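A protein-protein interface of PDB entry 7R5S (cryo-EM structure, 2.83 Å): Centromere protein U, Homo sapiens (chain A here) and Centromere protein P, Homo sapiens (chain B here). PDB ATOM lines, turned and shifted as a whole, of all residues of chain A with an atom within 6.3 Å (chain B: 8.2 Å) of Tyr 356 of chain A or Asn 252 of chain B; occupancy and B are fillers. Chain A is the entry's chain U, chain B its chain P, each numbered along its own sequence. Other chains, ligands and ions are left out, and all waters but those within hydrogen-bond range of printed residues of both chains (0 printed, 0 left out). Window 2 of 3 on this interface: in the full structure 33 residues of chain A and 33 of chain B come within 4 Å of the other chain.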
ATOM      1  N   LEU A 351      15.395  19.095  11.046  1.00  0.00           N
ATOM      2  CA  LEU A 351      14.964  18.413   9.829  1.00  0.00           C
ATOM      3  C   LEU A 351      14.608  16.958  10.110  1.00  0.00           C
ATOM      4  O   LEU A 351      13.570  16.463   9.651  1.00  0.00           O
ATOM      5  CB  LEU A 351      16.057  18.508   8.763  1.00  0.00           C
ATOM      6  CG  LEU A 351      15.793  17.845   7.409  1.00  0.00           C
ATOM      7  CD1 LEU A 351      16.258  18.749   6.279  1.00  0.00           C
ATOM      8  CD2 LEU A 351      16.487  16.494   7.323  1.00  0.00           C
ATOM      9  N   ARG A 352      15.458  16.259  10.869  1.00  0.00           N
ATOM     10  CA  ARG A 352      15.182  14.861  11.188  1.00  0.00           C
ATOM     11  C   ARG A 352      13.901  14.721  12.002  1.00  0.00           C
ATOM     12  O   ARG A 352      13.074  13.838  11.729  1.00  0.00           O
ATOM     13  CB  ARG A 352      16.365  14.251  11.939  1.00  0.00           C
ATOM     14  CG  ARG A 352      16.131  12.826  12.416  1.00  0.00           C
ATOM     15  CD  ARG A 352      17.052  12.472  13.573  1.00  0.00           C
ATOM     16  NE  ARG A 352      16.843  13.341  14.727  1.00  0.00           N
ATOM     17  CZ  ARG A 352      15.940  13.119  15.676  1.00  0.00           C
ATOM     18  NH1 ARG A 352      15.157  12.051  15.612  1.00  0.00           N
ATOM     19  NH2 ARG A 352      15.820  13.964  16.691  1.00  0.00           N
ATOM     20  N   ASN A 353      13.720  15.583  13.008  1.00  0.00           N
ATOM     21  CA  ASN A 353      12.512  15.514  13.828  1.00  0.00           C
ATOM     22  C   ASN A 353      11.260  15.754  12.990  1.00  0.00           C
ATOM     23  O   ASN A 353      10.257  15.040  13.133  1.00  0.00           O
ATOM     24  CB  ASN A 353      12.600  16.524  14.972  1.00  0.00           C
ATOM     25  CG  ASN A 353      11.619  16.229  16.093  1.00  0.00           C
ATOM     26  OD1 ASN A 353      10.447  15.938  15.853  1.00  0.00           O
ATOM     27  ND2 ASN A 353      12.099  16.304  17.330  1.00  0.00           N
ATOM     28  N   ALA A 354      11.301  16.762  12.111  1.00  0.00           N
ATOM     29  CA  ALA A 354      10.149  17.057  11.268  1.00  0.00           C
ATOM     30  C   ALA A 354       9.838  15.897  10.333  1.00  0.00           C
ATOM     31  O   ALA A 354       8.667  15.543  10.142  1.00  0.00           O
ATOM     32  CB  ALA A 354      10.393  18.338  10.473  1.00  0.00           C
ATOM     33  N   ALA A 355      10.870  15.292   9.738  1.00  0.00           N
ATOM     34  CA  ALA A 355      10.651  14.147   8.861  1.00  0.00           C
ATOM     35  C   ALA A 355       9.998  12.996   9.617  1.00  0.00           C
ATOM     36  O   ALA A 355       9.049  12.370   9.124  1.00  0.00           O
ATOM     37  CB  ALA A 355      11.973  13.700   8.240  1.00  0.00           C
ATOM     38  N   TYR A 356      10.498  12.704  10.821  1.00  0.00           N
ATOM     39  CA  TYR A 356       9.932  11.614  11.611  1.00  0.00           C
ATOM     40  C   TYR A 356       8.464  11.872  11.928  1.00  0.00           C
ATOM     41  O   TYR A 356       7.612  10.993  11.744  1.00  0.00           O
ATOM     42  CB  TYR A 356      10.739  11.422  12.895  1.00  0.00           C
ATOM     43  CG  TYR A 356      10.115  10.446  13.869  1.00  0.00           C
ATOM     44  CD1 TYR A 356      10.163   9.078  13.638  1.00  0.00           C
ATOM     45  CD2 TYR A 356       9.482  10.894  15.021  1.00  0.00           C
ATOM     46  CE1 TYR A 356       9.595   8.182  14.525  1.00  0.00           C
ATOM     47  CE2 TYR A 356       8.912  10.006  15.915  1.00  0.00           C
ATOM     48  CZ  TYR A 356       8.971   8.653  15.662  1.00  0.00           C
ATOM     49  OH  TYR A 356       8.405   7.765  16.548  1.00  0.00           O
ATOM     50  N   PHE A 357       8.149  13.081  12.403  1.00  0.00           N
ATOM     51  CA  PHE A 357       6.767  13.393  12.762  1.00  0.00           C
ATOM     52  C   PHE A 357       5.852  13.326  11.543  1.00  0.00           C
ATOM     53  O   PHE A 357       4.730  12.805  11.620  1.00  0.00           O
ATOM     54  CB  PHE A 357       6.690  14.772  13.417  1.00  0.00           C
ATOM     55  CG  PHE A 357       5.292  15.316  13.522  1.00  0.00           C
ATOM     56  CD1 PHE A 357       4.430  14.860  14.505  1.00  0.00           C
ATOM     57  CD2 PHE A 357       4.840  16.282  12.636  1.00  0.00           C
ATOM     58  CE1 PHE A 357       3.144  15.357  14.605  1.00  0.00           C
ATOM     59  CE2 PHE A 357       3.554  16.781  12.730  1.00  0.00           C
ATOM     60  CZ  PHE A 357       2.706  16.318  13.716  1.00  0.00           C
ATOM     61  N   LEU A 358       6.315  13.853  10.407  1.00  0.00           N
ATOM     62  CA  LEU A 358       5.493  13.854   9.201  1.00  0.00           C
ATOM     63  C   LEU A 358       5.207  12.434   8.732  1.00  0.00           C
ATOM     64  O   LEU A 358       4.064  12.099   8.400  1.00  0.00           O
ATOM     65  CB  LEU A 358       6.181  14.662   8.099  1.00  0.00           C
ATOM     66  CG  LEU A 358       5.255  15.392   7.124  1.00  0.00           C
ATOM     67  CD1 LEU A 358       4.256  16.257   7.878  1.00  0.00           C
ATOM     68  CD2 LEU A 358       6.060  16.230   6.144  1.00  0.00           C
ATOM     69  N   SER A 359       6.236  11.582   8.698  1.00  0.00           N
ATOM     70  CA  SER A 359       6.024  10.197   8.284  1.00  0.00           C
ATOM     71  C   SER A 359       5.087   9.473   9.243  1.00  0.00           C
ATOM     72  O   SER A 359       4.214   8.705   8.814  1.00  0.00           O
ATOM     73  CB  SER A 359       7.363   9.467   8.188  1.00  0.00           C
ATOM     74  OG  SER A 359       7.731   8.912   9.440  1.00  0.00           O
ATOM     75  N   ASN A 360       5.250   9.711  10.548  1.00  0.00           N
ATOM     76  CA  ASN A 360       4.397   9.057  11.535  1.00  0.00           C
ATOM     77  C   ASN A 360       2.938   9.443  11.330  1.00  0.00           C
ATOM     78  O   ASN A 360       2.056   8.576  11.283  1.00  0.00           O
ATOM     79  CB  ASN A 360       4.869   9.422  12.945  1.00  0.00           C
ATOM     80  CG  ASN A 360       4.210   8.580  14.028  1.00  0.00           C
ATOM     81  OD1 ASN A 360       3.141   8.003  13.832  1.00  0.00           O
ATOM     82  ND2 ASN A 360       4.855   8.514  15.187  1.00  0.00           N
ATOM     83  N   LEU A 361       2.664  10.744  11.192  1.00  0.00           N
ATOM     84  CA  LEU A 361       1.284  11.185  10.996  1.00  0.00           C
ATOM     85  C   LEU A 361       0.721  10.695   9.666  1.00  0.00           C
ATOM     86  O   LEU A 361      -0.464  10.341   9.587  1.00  0.00           O
ATOM     87  CB  LEU A 361       1.203  12.710  11.099  1.00  0.00           C
ATOM     88  CG  LEU A 361      -0.110  13.430  10.770  1.00  0.00           C
ATOM     89  CD1 LEU A 361      -0.253  14.667  11.638  1.00  0.00           C
ATOM     90  CD2 LEU A 361      -0.184  13.826   9.299  1.00  0.00           C
ATOM     91  N   ALA B 246      -9.066   7.277  16.981  1.00  0.00           N
ATOM     92  CA  ALA B 246      -7.667   7.351  16.577  1.00  0.00           C
ATOM     93  C   ALA B 246      -6.722   7.307  17.769  1.00  0.00           C
ATOM     94  O   ALA B 246      -5.560   6.920  17.608  1.00  0.00           O
ATOM     95  CB  ALA B 246      -7.417   8.617  15.760  1.00  0.00           C
ATOM     96  N   LEU B 247      -7.192   7.696  18.955  1.00  0.00           N
ATOM     97  CA  LEU B 247      -6.355   7.628  20.147  1.00  0.00           C
ATOM     98  C   LEU B 247      -6.287   6.206  20.695  1.00  0.00           C
ATOM     99  O   LEU B 247      -5.221   5.756  21.129  1.00  0.00           O
ATOM    100  CB  LEU B 247      -6.879   8.594  21.212  1.00  0.00           C
ATOM    101  CG  LEU B 247      -5.862   9.178  22.196  1.00  0.00           C
ATOM    102  CD1 LEU B 247      -6.342  10.526  22.710  1.00  0.00           C
ATOM    103  CD2 LEU B 247      -5.601   8.229  23.358  1.00  0.00           C
ATOM    104  N   LEU B 249      -6.692   3.653  18.812  1.00  0.00           N
ATOM    105  CA  LEU B 249      -6.042   2.873  17.763  1.00  0.00           C
ATOM    106  C   LEU B 249      -4.525   2.957  17.877  1.00  0.00           C
ATOM    107  O   LEU B 249      -3.831   1.934  17.849  1.00  0.00           O
ATOM    108  CB  LEU B 249      -6.523   3.356  16.390  1.00  0.00           C
ATOM    109  CG  LEU B 249      -6.051   2.693  15.090  1.00  0.00           C
ATOM    110  CD1 LEU B 249      -7.064   2.951  13.987  1.00  0.00           C
ATOM    111  CD2 LEU B 249      -4.686   3.206  14.654  1.00  0.00           C
ATOM    112  N   ASP B 250      -3.990   4.169  18.007  1.00  0.00           N
ATOM    113  CA  ASP B 250      -2.552   4.401  18.006  1.00  0.00           C
ATOM    114  C   ASP B 250      -2.063   4.604  19.434  1.00  0.00           C
ATOM    115  O   ASP B 250      -2.574   5.468  20.154  1.00  0.00           O
ATOM    116  CB  ASP B 250      -2.198   5.612  17.142  1.00  0.00           C
ATOM    117  CG  ASP B 250      -0.736   6.000  17.254  1.00  0.00           C
ATOM    118  OD1 ASP B 250       0.122   5.260  16.728  1.00  0.00           O
ATOM    119  OD2 ASP B 250      -0.443   7.048  17.869  1.00  0.00           O
ATOM    120  N   LYS B 251      -1.078   3.805  19.839  1.00  0.00           N
ATOM    121  CA  LYS B 251      -0.434   3.944  21.137  1.00  0.00           C
ATOM    122  C   LYS B 251       0.920   4.637  21.053  1.00  0.00           C
ATOM    123  O   LYS B 251       1.589   4.784  22.080  1.00  0.00           O
ATOM    124  CB  LYS B 251      -0.270   2.570  21.797  1.00  0.00           C
ATOM    125  CG  LYS B 251      -1.579   1.834  22.019  1.00  0.00           C
ATOM    126  CD  LYS B 251      -2.395   2.502  23.114  1.00  0.00           C
ATOM    127  CE  LYS B 251      -3.869   2.556  22.757  1.00  0.00           C
ATOM    128  NZ  LYS B 251      -4.147   3.649  21.786  1.00  0.00           N
ATOM    129  N   ASN B 252       1.341   5.058  19.858  1.00  0.00           N
ATOM    130  CA  ASN B 252       2.613   5.761  19.734  1.00  0.00           C
ATOM    131  C   ASN B 252       2.531   7.170  20.308  1.00  0.00           C
ATOM    132  O   ASN B 252       3.554   7.725  20.724  1.00  0.00           O
ATOM    133  CB  ASN B 252       3.050   5.802  18.269  1.00  0.00           C
ATOM    134  CG  ASN B 252       4.547   5.973  18.113  1.00  0.00           C
ATOM    135  OD1 ASN B 252       5.285   6.008  19.098  1.00  0.00           O
ATOM    136  ND2 ASN B 252       5.005   6.069  16.871  1.00  0.00           N
ATOM    137  N   ARG B 253       1.332   7.755  20.336  1.00  0.00           N
ATOM    138  CA  ARG B 253       1.074   9.058  20.951  1.00  0.00           C
ATOM    139  C   ARG B 253       1.951  10.147  20.322  1.00  0.00           C
ATOM    140  O   ARG B 253       2.808  10.757  20.964  1.00  0.00           O
ATOM    141  CB  ARG B 253       1.269   8.992  22.470  1.00  0.00           C
ATOM    142  CG  ARG B 253       0.538   7.840  23.143  1.00  0.00           C
ATOM    143  CD  ARG B 253      -0.959   7.888  22.871  1.00  0.00           C
ATOM    144  NE  ARG B 253      -1.581   9.094  23.410  1.00  0.00           N
ATOM    145  CZ  ARG B 253      -2.136  10.045  22.666  1.00  0.00           C
ATOM    146  NH1 ARG B 253      -2.156   9.929  21.345  1.00  0.00           N
ATOM    147  NH2 ARG B 253      -2.679  11.109  23.241  1.00  0.00           N
ATOM    148  N   ALA B 254       1.704  10.373  19.033  1.00  0.00           N
ATOM    149  CA  ALA B 254       2.421  11.380  18.262  1.00  0.00           C
ATOM    150  C   ALA B 254       1.529  12.537  17.828  1.00  0.00           C
ATOM    151  O   ALA B 254       1.901  13.281  16.915  1.00  0.00           O
ATOM    152  CB  ALA B 254       3.079  10.740  17.039  1.00  0.00           C
ATOM    153  N   ILE B 255       0.364  12.709  18.452  1.00  0.00           N
ATOM    154  CA  ILE B 255      -0.568  13.755  18.042  1.00  0.00           C
ATOM    155  C   ILE B 255      -0.563  14.901  19.047  1.00  0.00           C
ATOM    156  O   ILE B 255      -0.733  16.066  18.669  1.00  0.00           O
ATOM    157  CB  ILE B 255      -1.988  13.191  17.852  1.00  0.00           C
ATOM    158  CG1 ILE B 255      -2.391  12.318  19.044  1.00  0.00           C
ATOM    159  CG2 ILE B 255      -2.080  12.405  16.553  1.00  0.00           C
ATOM    160  CD1 ILE B 255      -3.317  13.007  20.025  1.00  0.00           C
ATOM    161  N   GLU B 256      -0.365  14.587  20.331  1.00  0.00           N
ATOM    162  CA  GLU B 256      -0.371  15.638  21.343  1.00  0.00           C
ATOM    163  C   GLU B 256       0.824  16.569  21.192  1.00  0.00           C
ATOM    164  O   GLU B 256       0.744  17.745  21.567  1.00  0.00           O
ATOM    165  CB  GLU B 256      -0.398  15.032  22.747  1.00  0.00           C
ATOM    166  CG  GLU B 256       0.819  14.194  23.096  1.00  0.00           C
ATOM    167  CD  GLU B 256       0.636  12.734  22.745  1.00  0.00           C
ATOM    168  OE1 GLU B 256       0.401  12.430  21.557  1.00  0.00           O
ATOM    169  OE2 GLU B 256       0.725  11.889  23.661  1.00  0.00           O
ATOM    170  N   THR B 257       1.934  16.069  20.649  1.00  0.00           N
ATOM    171  CA  THR B 257       3.084  16.893  20.313  1.00  0.00           C
ATOM    172  C   THR B 257       3.000  17.454  18.899  1.00  0.00           C
ATOM    173  O   THR B 257       4.008  17.935  18.367  1.00  0.00           O
ATOM    174  CB  THR B 257       4.377  16.091  20.488  1.00  0.00           C
ATOM    175  OG1 THR B 257       5.506  16.966  20.362  1.00  0.00           O
ATOM    176  CG2 THR B 257       4.470  14.984  19.445  1.00  0.00           C
ATOM    177  N   SER B 261       5.886  20.462  17.139  1.00  0.00           N
ATOM    178  CA  SER B 261       6.586  19.931  15.973  1.00  0.00           C
ATOM    179  C   SER B 261       6.166  20.657  14.702  1.00  0.00           C
ATOM    180  O   SER B 261       7.006  20.994  13.858  1.00  0.00           O
ATOM    181  CB  SER B 261       6.325  18.429  15.849  1.00  0.00           C
ATOM    182  OG  SER B 261       5.130  18.180  15.131  1.00  0.00           O
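The side-chain amide nitrogen (ND2) of Asn 360 of chain A sits close to the side-chain amide nitrogen (ND2) of Asn 252 of chain B.
ND2 of Asn 252 of chain B touches OH of Tyr 356 of chain A, 3.8 Å away. CE1 of Phe 357 of chain A touches O of Ala 254 of chain B, 3.3 Å away. Ser 261 of chain B touches Phe 357 of chain A (OG to CD2, 3.1 Å). ND2 of Asn 360 of chain A touches CB of Ala 254 of chain B, at 3.4 Å.
Printed residues of chain B that touch a printed residue of chain A: Asn 252, Ala 254 and Ser 261. Hydrophobic or aromatic side chains of chain A that line the printed part of chain B: Tyr 356 and Phe 357. Among the printed residues, no Asp or Glu carboxylate lies within 4 Å of a Lys or Arg side-chain nitrogen of the other chain.
Ala 355 of chain A touches none of the printed residues of chain B. Printed residues of chain B within 4 Å of Tyr 356 of chain A: Asn 252. Of the printed residues of chain B, Asn 360 of chain A touches Asn 252 (3.0 Å) and Ala 254 (3.4 Å). Asn 252 of chain B touches just these residues of chain A: Tyr 356 and Asn 360. Of the printed residues of chain A, Ala 254 of chain B touches Phe 357 and Asn 360. The nearest printed residue of chain A that does not touch Asn 252 of chain B is Leu 361 of chain A (7.7 Å).
The side-chain hydroxyl (OG) of Ser 359 of chain A sits at hydrogen-bond distance from the backbone carbonyl oxygen (O) of Tyr 356 of chain A, at 3.1 Å. OD2 of Asp 250 of chain B is in hydrogen-bond range of N of Asn 252 of chain B, 3.3 Å away. The backbone carbonyl oxygen of Thr 257 of chain B sits at hydrogen-bond distance from the side-chain hydroxyl of Ser 261 of chain B (3.4 Å).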
